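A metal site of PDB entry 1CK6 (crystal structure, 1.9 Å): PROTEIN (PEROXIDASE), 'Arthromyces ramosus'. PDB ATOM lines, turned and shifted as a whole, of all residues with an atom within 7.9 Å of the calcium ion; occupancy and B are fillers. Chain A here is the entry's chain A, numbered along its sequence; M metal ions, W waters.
Water W1 lies within hydrogen-bond range of OE1 of Glu 87 (2.8 Å) and O of His 56 (3.0 Å).
The side-chain carboxylate (OD1) of Asp 57 binds the calcium ion, at 2.3 Å.
The calcium ion is bound by OD1 of Asp 77 (2.5 Å).
The calcium ion is bound by water W2 (2.5 Å).
O of Asp 57 binds the calcium ion.
The calcium ion is bound by the backbone carbonyl oxygen (O) of Gly 75, at 2.6 Å.
The calcium ion is bound by the side-chain hydroxyl (OG) of Ser 79 (2.6 Å).
The calcium ion is bound by water W1 (2.7 Å).
The backbone NH of Gly 78 is in hydrogen-bond range of the side-chain carboxylate of Asp 57 (2.9 Å).
N of Gly 75 is in hydrogen-bond range of O of Gly 60.
The side-chain hydroxyl (OG) of Ser 79 lies close to the side-chain carboxylate (OE2) of Glu 87, at 2.7 Å.
Of the 29 residues printed, 4 come within 4 Å of the calcium ion.
The nearest printed residue that does not touch the calcium ion is Gly 78 (4.5 Å).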
ATOM      1  N   ILE A  53     -23.117  31.755 -11.599  1.00  0.00           N
ATOM      2  CA  ILE A  53     -23.397  30.465 -12.219  1.00  0.00           C
ATOM      3  C   ILE A  53     -22.140  29.734 -12.698  1.00  0.00           C
ATOM      4  O   ILE A  53     -22.035  28.522 -12.470  1.00  0.00           O
ATOM      5  CB  ILE A  53     -24.403  30.687 -13.393  1.00  0.00           C
ATOM      6  CG1 ILE A  53     -25.792  30.937 -12.784  1.00  0.00           C
ATOM      7  CG2 ILE A  53     -24.467  29.485 -14.338  1.00  0.00           C
ATOM      8  CD1 ILE A  53     -26.790  31.488 -13.831  1.00  0.00           C
ATOM      9  N   VAL A  54     -21.139  30.383 -13.310  1.00  0.00           N
ATOM     10  CA  VAL A  54     -19.969  29.660 -13.843  1.00  0.00           C
ATOM     11  C   VAL A  54     -19.157  29.027 -12.711  1.00  0.00           C
ATOM     12  O   VAL A  54     -18.682  27.881 -12.788  1.00  0.00           O
ATOM     13  CB  VAL A  54     -19.179  30.694 -14.733  1.00  0.00           C
ATOM     14  CG1 VAL A  54     -18.342  31.708 -13.940  1.00  0.00           C
ATOM     15  CG2 VAL A  54     -18.295  29.872 -15.635  1.00  0.00           C
ATOM     16  N   PHE A  55     -19.107  29.734 -11.585  1.00  0.00           N
ATOM     17  CA  PHE A  55     -18.454  29.264 -10.380  1.00  0.00           C
ATOM     18  C   PHE A  55     -19.277  28.099  -9.862  1.00  0.00           C
ATOM     19  O   PHE A  55     -18.699  27.023  -9.689  1.00  0.00           O
ATOM     20  CB  PHE A  55     -18.386  30.383  -9.291  1.00  0.00           C
ATOM     21  CG  PHE A  55     -17.811  29.939  -7.941  1.00  0.00           C
ATOM     22  CD1 PHE A  55     -16.685  29.104  -7.853  1.00  0.00           C
ATOM     23  CD2 PHE A  55     -18.426  30.358  -6.760  1.00  0.00           C
ATOM     24  CE1 PHE A  55     -16.188  28.693  -6.616  1.00  0.00           C
ATOM     25  CE2 PHE A  55     -17.938  29.951  -5.525  1.00  0.00           C
ATOM     26  CZ  PHE A  55     -16.820  29.118  -5.453  1.00  0.00           C
ATOM     27  N   HIS A  56     -20.597  28.199  -9.681  1.00  0.00           N
ATOM     28  CA  HIS A  56     -21.357  27.092  -9.110  1.00  0.00           C
ATOM     29  C   HIS A  56     -21.400  25.845  -9.970  1.00  0.00           C
ATOM     30  O   HIS A  56     -21.539  24.703  -9.485  1.00  0.00           O
ATOM     31  CB  HIS A  56     -22.791  27.579  -8.780  1.00  0.00           C
ATOM     32  CG  HIS A  56     -22.808  28.547  -7.594  1.00  0.00           C
ATOM     33  ND1 HIS A  56     -23.950  28.965  -6.928  1.00  0.00           N
ATOM     34  CD2 HIS A  56     -21.669  29.131  -6.995  1.00  0.00           C
ATOM     35  CE1 HIS A  56     -23.506  29.779  -5.935  1.00  0.00           C
ATOM     36  NE2 HIS A  56     -22.212  29.877  -5.945  1.00  0.00           N
ATOM     37  N   ASP A  57     -21.267  26.054 -11.269  1.00  0.00           N
ATOM     38  CA  ASP A  57     -21.206  24.936 -12.193  1.00  0.00           C
ATOM     39  C   ASP A  57     -19.829  24.271 -12.141  1.00  0.00           C
ATOM     40  O   ASP A  57     -19.776  23.054 -11.876  1.00  0.00           O
ATOM     41  CB  ASP A  57     -21.467  25.370 -13.646  1.00  0.00           C
ATOM     42  CG  ASP A  57     -21.454  24.216 -14.651  1.00  0.00           C
ATOM     43  OD1 ASP A  57     -21.828  23.101 -14.283  1.00  0.00           O
ATOM     44  OD2 ASP A  57     -21.081  24.420 -15.799  1.00  0.00           O
ATOM     45  N   ALA A  58     -18.729  25.032 -12.294  1.00  0.00           N
ATOM     46  CA  ALA A  58     -17.411  24.446 -12.335  1.00  0.00           C
ATOM     47  C   ALA A  58     -16.919  23.852 -11.039  1.00  0.00           C
ATOM     48  O   ALA A  58     -16.245  22.833 -11.089  1.00  0.00           O
ATOM     49  CB  ALA A  58     -16.396  25.469 -12.796  1.00  0.00           C
ATOM     50  N   ILE A  59     -17.265  24.432  -9.891  1.00  0.00           N
ATOM     51  CA  ILE A  59     -16.795  23.934  -8.599  1.00  0.00           C
ATOM     52  C   ILE A  59     -17.446  22.607  -8.158  1.00  0.00           C
ATOM     53  O   ILE A  59     -16.965  22.022  -7.178  1.00  0.00           O
ATOM     54  CB  ILE A  59     -16.975  25.114  -7.524  1.00  0.00           C
ATOM     55  CG1 ILE A  59     -15.912  24.978  -6.458  1.00  0.00           C
ATOM     56  CG2 ILE A  59     -18.333  25.065  -6.790  1.00  0.00           C
ATOM     57  CD1 ILE A  59     -14.487  25.174  -6.983  1.00  0.00           C
ATOM     58  N   GLY A  60     -18.501  22.068  -8.801  1.00  0.00           N
ATOM     59  CA  GLY A  60     -19.075  20.798  -8.399  1.00  0.00           C
ATOM     60  C   GLY A  60     -18.138  19.781  -9.026  1.00  0.00           C
ATOM     61  O   GLY A  60     -18.404  19.186 -10.082  1.00  0.00           O
ATOM     62  N   PHE A  61     -16.983  19.633  -8.406  1.00  0.00           N
ATOM     63  CA  PHE A  61     -15.923  18.783  -8.905  1.00  0.00           C
ATOM     64  C   PHE A  61     -15.088  18.479  -7.665  1.00  0.00           C
ATOM     65  O   PHE A  61     -14.581  19.399  -7.025  1.00  0.00           O
ATOM     66  CB  PHE A  61     -15.138  19.578  -9.958  1.00  0.00           C
ATOM     67  CG  PHE A  61     -13.938  18.826 -10.485  1.00  0.00           C
ATOM     68  CD1 PHE A  61     -14.129  17.780 -11.374  1.00  0.00           C
ATOM     69  CD2 PHE A  61     -12.648  19.192 -10.062  1.00  0.00           C
ATOM     70  CE1 PHE A  61     -13.022  17.088 -11.846  1.00  0.00           C
ATOM     71  CE2 PHE A  61     -11.544  18.494 -10.541  1.00  0.00           C
ATOM     72  CZ  PHE A  61     -11.727  17.436 -11.436  1.00  0.00           C
ATOM     73  N   GLY A  73     -18.420  14.691  -9.385  1.00  0.00           N
ATOM     74  CA  GLY A  73     -18.939  15.843 -10.101  1.00  0.00           C
ATOM     75  C   GLY A  73     -18.168  16.034 -11.406  1.00  0.00           C
ATOM     76  O   GLY A  73     -17.010  15.647 -11.472  1.00  0.00           O
ATOM     77  N   GLY A  74     -18.744  16.584 -12.452  1.00  0.00           N
ATOM     78  CA  GLY A  74     -18.037  16.752 -13.698  1.00  0.00           C
ATOM     79  C   GLY A  74     -17.390  18.129 -13.908  1.00  0.00           C
ATOM     80  O   GLY A  74     -16.909  18.385 -15.025  1.00  0.00           O
ATOM     81  N   GLY A  75     -17.356  19.055 -12.947  1.00  0.00           N
ATOM     82  CA  GLY A  75     -16.714  20.340 -13.177  1.00  0.00           C
ATOM     83  C   GLY A  75     -17.532  21.234 -14.091  1.00  0.00           C
ATOM     84  O   GLY A  75     -18.774  21.320 -13.950  1.00  0.00           O
ATOM     85  N   ALA A  76     -16.874  21.882 -15.053  1.00  0.00           N
ATOM     86  CA  ALA A  76     -17.494  22.816 -15.968  1.00  0.00           C
ATOM     87  C   ALA A  76     -18.269  22.135 -17.086  1.00  0.00           C
ATOM     88  O   ALA A  76     -18.087  22.419 -18.271  1.00  0.00           O
ATOM     89  CB  ALA A  76     -16.390  23.713 -16.578  1.00  0.00           C
ATOM     90  N   ASP A  77     -19.257  21.315 -16.698  1.00  0.00           N
ATOM     91  CA  ASP A  77     -20.044  20.516 -17.598  1.00  0.00           C
ATOM     92  C   ASP A  77     -21.456  20.976 -17.943  1.00  0.00           C
ATOM     93  O   ASP A  77     -22.193  20.263 -18.637  1.00  0.00           O
ATOM     94  CB  ASP A  77     -20.077  19.086 -17.009  1.00  0.00           C
ATOM     95  CG  ASP A  77     -20.742  19.028 -15.639  1.00  0.00           C
ATOM     96  OD1 ASP A  77     -21.300  20.017 -15.164  1.00  0.00           O
ATOM     97  OD2 ASP A  77     -20.729  17.975 -15.015  1.00  0.00           O
ATOM     98  N   GLY A  78     -21.892  22.129 -17.411  1.00  0.00           N
ATOM     99  CA  GLY A  78     -23.264  22.652 -17.628  1.00  0.00           C
ATOM    100  C   GLY A  78     -24.343  21.857 -16.882  1.00  0.00           C
ATOM    101  O   GLY A  78     -25.540  21.992 -17.148  1.00  0.00           O
ATOM    102  N   SER A  79     -23.951  21.096 -15.854  1.00  0.00           N
ATOM    103  CA  SER A  79     -24.899  20.262 -15.138  1.00  0.00           C
ATOM    104  C   SER A  79     -25.862  21.132 -14.365  1.00  0.00           C
ATOM    105  O   SER A  79     -26.978  20.687 -14.108  1.00  0.00           O
ATOM    106  CB  SER A  79     -24.191  19.320 -14.169  1.00  0.00           C
ATOM    107  OG  SER A  79     -23.458  20.016 -13.158  1.00  0.00           O
ATOM    108  N   ILE A  80     -25.486  22.377 -13.980  1.00  0.00           N
ATOM    109  CA  ILE A  80     -26.413  23.250 -13.281  1.00  0.00           C
ATOM    110  C   ILE A  80     -27.612  23.589 -14.175  1.00  0.00           C
ATOM    111  O   ILE A  80     -28.687  23.908 -13.649  1.00  0.00           O
ATOM    112  CB  ILE A  80     -25.599  24.490 -12.792  1.00  0.00           C
ATOM    113  CG1 ILE A  80     -26.436  25.278 -11.795  1.00  0.00           C
ATOM    114  CG2 ILE A  80     -25.148  25.358 -13.979  1.00  0.00           C
ATOM    115  CD1 ILE A  80     -25.654  26.355 -11.037  1.00  0.00           C
ATOM    116  N   ILE A  81     -27.510  23.475 -15.511  1.00  0.00           N
ATOM    117  CA  ILE A  81     -28.633  23.707 -16.421  1.00  0.00           C
ATOM    118  C   ILE A  81     -29.278  22.350 -16.707  1.00  0.00           C
ATOM    119  O   ILE A  81     -30.475  22.184 -16.464  1.00  0.00           O
ATOM    120  CB  ILE A  81     -28.163  24.327 -17.739  1.00  0.00           C
ATOM    121  CG1 ILE A  81     -27.448  25.659 -17.478  1.00  0.00           C
ATOM    122  CG2 ILE A  81     -29.383  24.496 -18.641  1.00  0.00           C
ATOM    123  CD1 ILE A  81     -27.021  26.418 -18.750  1.00  0.00           C
ATOM    124  N   HIS A  83     -29.294  19.584 -15.094  1.00  0.00           N
ATOM    125  CA  HIS A  83     -29.840  19.003 -13.881  1.00  0.00           C
ATOM    126  C   HIS A  83     -30.251  20.136 -12.952  1.00  0.00           C
ATOM    127  O   HIS A  83     -30.080  20.001 -11.737  1.00  0.00           O
ATOM    128  CB  HIS A  83     -28.800  18.130 -13.178  1.00  0.00           C
ATOM    129  CG  HIS A  83     -28.450  17.039 -14.162  1.00  0.00           C
ATOM    130  ND1 HIS A  83     -29.337  16.047 -14.591  1.00  0.00           N
ATOM    131  CD2 HIS A  83     -27.233  16.952 -14.829  1.00  0.00           C
ATOM    132  CE1 HIS A  83     -28.642  15.358 -15.529  1.00  0.00           C
ATOM    133  NE2 HIS A  83     -27.454  15.852 -15.681  1.00  0.00           N
ATOM    134  N   GLU A  87     -29.783  20.574  -8.844  1.00  0.00           N
ATOM    135  CA  GLU A  87     -28.837  21.558  -8.321  1.00  0.00           C
ATOM    136  C   GLU A  87     -29.408  22.867  -7.821  1.00  0.00           C
ATOM    137  O   GLU A  87     -28.912  23.445  -6.850  1.00  0.00           O
ATOM    138  CB  GLU A  87     -27.802  21.854  -9.375  1.00  0.00           C
ATOM    139  CG  GLU A  87     -26.949  20.635  -9.585  1.00  0.00           C
ATOM    140  CD  GLU A  87     -25.757  20.896 -10.474  1.00  0.00           C
ATOM    141  OE1 GLU A  87     -25.193  21.993 -10.423  1.00  0.00           O
ATOM    142  OE2 GLU A  87     -25.397  19.981 -11.230  1.00  0.00           O
ATOM    143  N   GLY A 115     -22.178  23.359 -21.011  1.00  0.00           N
ATOM    144  CA  GLY A 115     -20.915  23.699 -20.361  1.00  0.00           C
ATOM    145  C   GLY A 115     -20.167  24.749 -21.149  1.00  0.00           C
ATOM    146  O   GLY A 115     -19.640  25.712 -20.576  1.00  0.00           O
ATOM    147  N   ILE A 118     -22.077  28.254 -20.835  1.00  0.00           N
ATOM    148  CA  ILE A 118     -21.845  29.028 -19.614  1.00  0.00           C
ATOM    149  C   ILE A 118     -20.474  29.712 -19.669  1.00  0.00           C
ATOM    150  O   ILE A 118     -20.394  30.893 -19.285  1.00  0.00           O
ATOM    151  CB  ILE A 118     -21.948  28.093 -18.364  1.00  0.00           C
ATOM    152  CG1 ILE A 118     -23.399  27.645 -18.176  1.00  0.00           C
ATOM    153  CG2 ILE A 118     -21.503  28.831 -17.114  1.00  0.00           C
ATOM    154  CD1 ILE A 118     -23.546  26.552 -17.103  1.00  0.00           C
ATOM    155  N   SER A 145     -23.866  15.257 -18.837  1.00  0.00           N
ATOM    156  CA  SER A 145     -23.403  15.421 -17.480  1.00  0.00           C
ATOM    157  C   SER A 145     -24.319  14.620 -16.528  1.00  0.00           C
ATOM    158  O   SER A 145     -25.375  14.061 -16.882  1.00  0.00           O
ATOM    159  CB  SER A 145     -23.428  16.900 -17.108  1.00  0.00           C
ATOM    160  OG  SER A 145     -24.717  17.463 -17.304  1.00  0.00           O
ATOM    161  N   GLN A 146     -23.798  14.494 -15.315  1.00  0.00           N
ATOM    162  CA  GLN A 146     -24.514  13.862 -14.233  1.00  0.00           C
ATOM    163  C   GLN A 146     -24.741  14.997 -13.260  1.00  0.00           C
ATOM    164  O   GLN A 146     -24.021  16.001 -13.339  1.00  0.00           O
ATOM    165  CB  GLN A 146     -23.635  12.795 -13.631  1.00  0.00           C
ATOM    166  CG  GLN A 146     -23.790  11.444 -14.302  1.00  0.00           C
ATOM    167  CD  GLN A 146     -22.495  10.666 -14.134  1.00  0.00           C
ATOM    168  OE1 GLN A 146     -21.576  10.822 -14.946  1.00  0.00           O
ATOM    169  NE2 GLN A 146     -22.336   9.834 -13.106  1.00  0.00           N
ATOM    170  N   PRO A 147     -25.683  14.943 -12.296  1.00  0.00           N
ATOM    171  CA  PRO A 147     -25.914  16.016 -11.345  1.00  0.00           C
ATOM    172  C   PRO A 147     -24.720  16.181 -10.429  1.00  0.00           C
ATOM    173  O   PRO A 147     -24.077  15.200 -10.050  1.00  0.00           O
ATOM    174  CB  PRO A 147     -27.170  15.600 -10.629  1.00  0.00           C
ATOM    175  CG  PRO A 147     -27.818  14.595 -11.535  1.00  0.00           C
ATOM    176  CD  PRO A 147     -26.602  13.844 -12.024  1.00  0.00           C
ATOM    177  N   SER A 148     -24.410  17.416 -10.072  1.00  0.00           N
ATOM    178  CA  SER A 148     -23.325  17.663  -9.148  1.00  0.00           C
ATOM    179  C   SER A 148     -23.706  17.080  -7.794  1.00  0.00           C
ATOM    180  O   SER A 148     -24.882  17.129  -7.412  1.00  0.00           O
ATOM    181  CB  SER A 148     -23.068  19.159  -8.958  1.00  0.00           C
ATOM    182  OG  SER A 148     -22.059  19.451  -7.983  1.00  0.00           O
ATOM    183  N   PRO A 149     -22.748  16.529  -7.045  1.00  0.00           N
ATOM    184  CA  PRO A 149     -22.952  16.122  -5.665  1.00  0.00           C
ATOM    185  C   PRO A 149     -23.272  17.417  -4.904  1.00  0.00           C
ATOM    186  O   PRO A 149     -22.872  18.519  -5.325  1.00  0.00           O
ATOM    187  CB  PRO A 149     -21.639  15.485  -5.280  1.00  0.00           C
ATOM    188  CG  PRO A 149     -21.174  14.866  -6.588  1.00  0.00           C
ATOM    189  CD  PRO A 149     -21.466  16.021  -7.528  1.00  0.00           C
ATOM    190  N   LEU A 283     -12.146  22.556 -15.436  1.00  0.00           N
ATOM    191  CA  LEU A 283     -12.241  21.547 -14.379  1.00  0.00           C
ATOM    192  C   LEU A 283     -13.165  20.420 -14.892  1.00  0.00           C
ATOM    193  O   LEU A 283     -14.266  20.650 -15.406  1.00  0.00           O
ATOM    194  CB  LEU A 283     -12.824  22.203 -13.131  1.00  0.00           C
ATOM    195  CG  LEU A 283     -12.009  22.495 -11.858  1.00  0.00           C
ATOM    196  CD1 LEU A 283     -10.621  23.016 -12.132  1.00  0.00           C
ATOM    197  CD2 LEU A 283     -12.824  23.486 -11.035  1.00  0.00           C
ATOM    198  N   PHE A 285     -12.142  18.510 -17.441  1.00  0.00           N
ATOM    199  CA  PHE A 285     -11.857  18.353 -18.865  1.00  0.00           C
ATOM    200  C   PHE A 285     -10.386  18.470 -19.084  1.00  0.00           C
ATOM    201  O   PHE A 285      -9.613  18.915 -18.209  1.00  0.00           O
ATOM    202  CB  PHE A 285     -12.496  19.446 -19.762  1.00  0.00           C
ATOM    203  CG  PHE A 285     -14.006  19.366 -19.674  1.00  0.00           C
ATOM    204  CD1 PHE A 285     -14.683  20.010 -18.637  1.00  0.00           C
ATOM    205  CD2 PHE A 285     -14.697  18.553 -20.589  1.00  0.00           C
ATOM    206  CE1 PHE A 285     -16.061  19.824 -18.493  1.00  0.00           C
ATOM    207  CE2 PHE A 285     -16.079  18.384 -20.448  1.00  0.00           C
ATOM    208  CZ  PHE A 285     -16.754  19.012 -19.395  1.00  0.00           C
HETATM  209 CA    CA M   1     -21.162  21.252 -13.032  1.00  0.00          CA
HETATM  210  O   HOH W   1     -22.447  22.141 -10.797  1.00  0.00           O
HETATM  211  O   HOH W   2     -20.610  19.414 -11.459  1.00  0.00           O
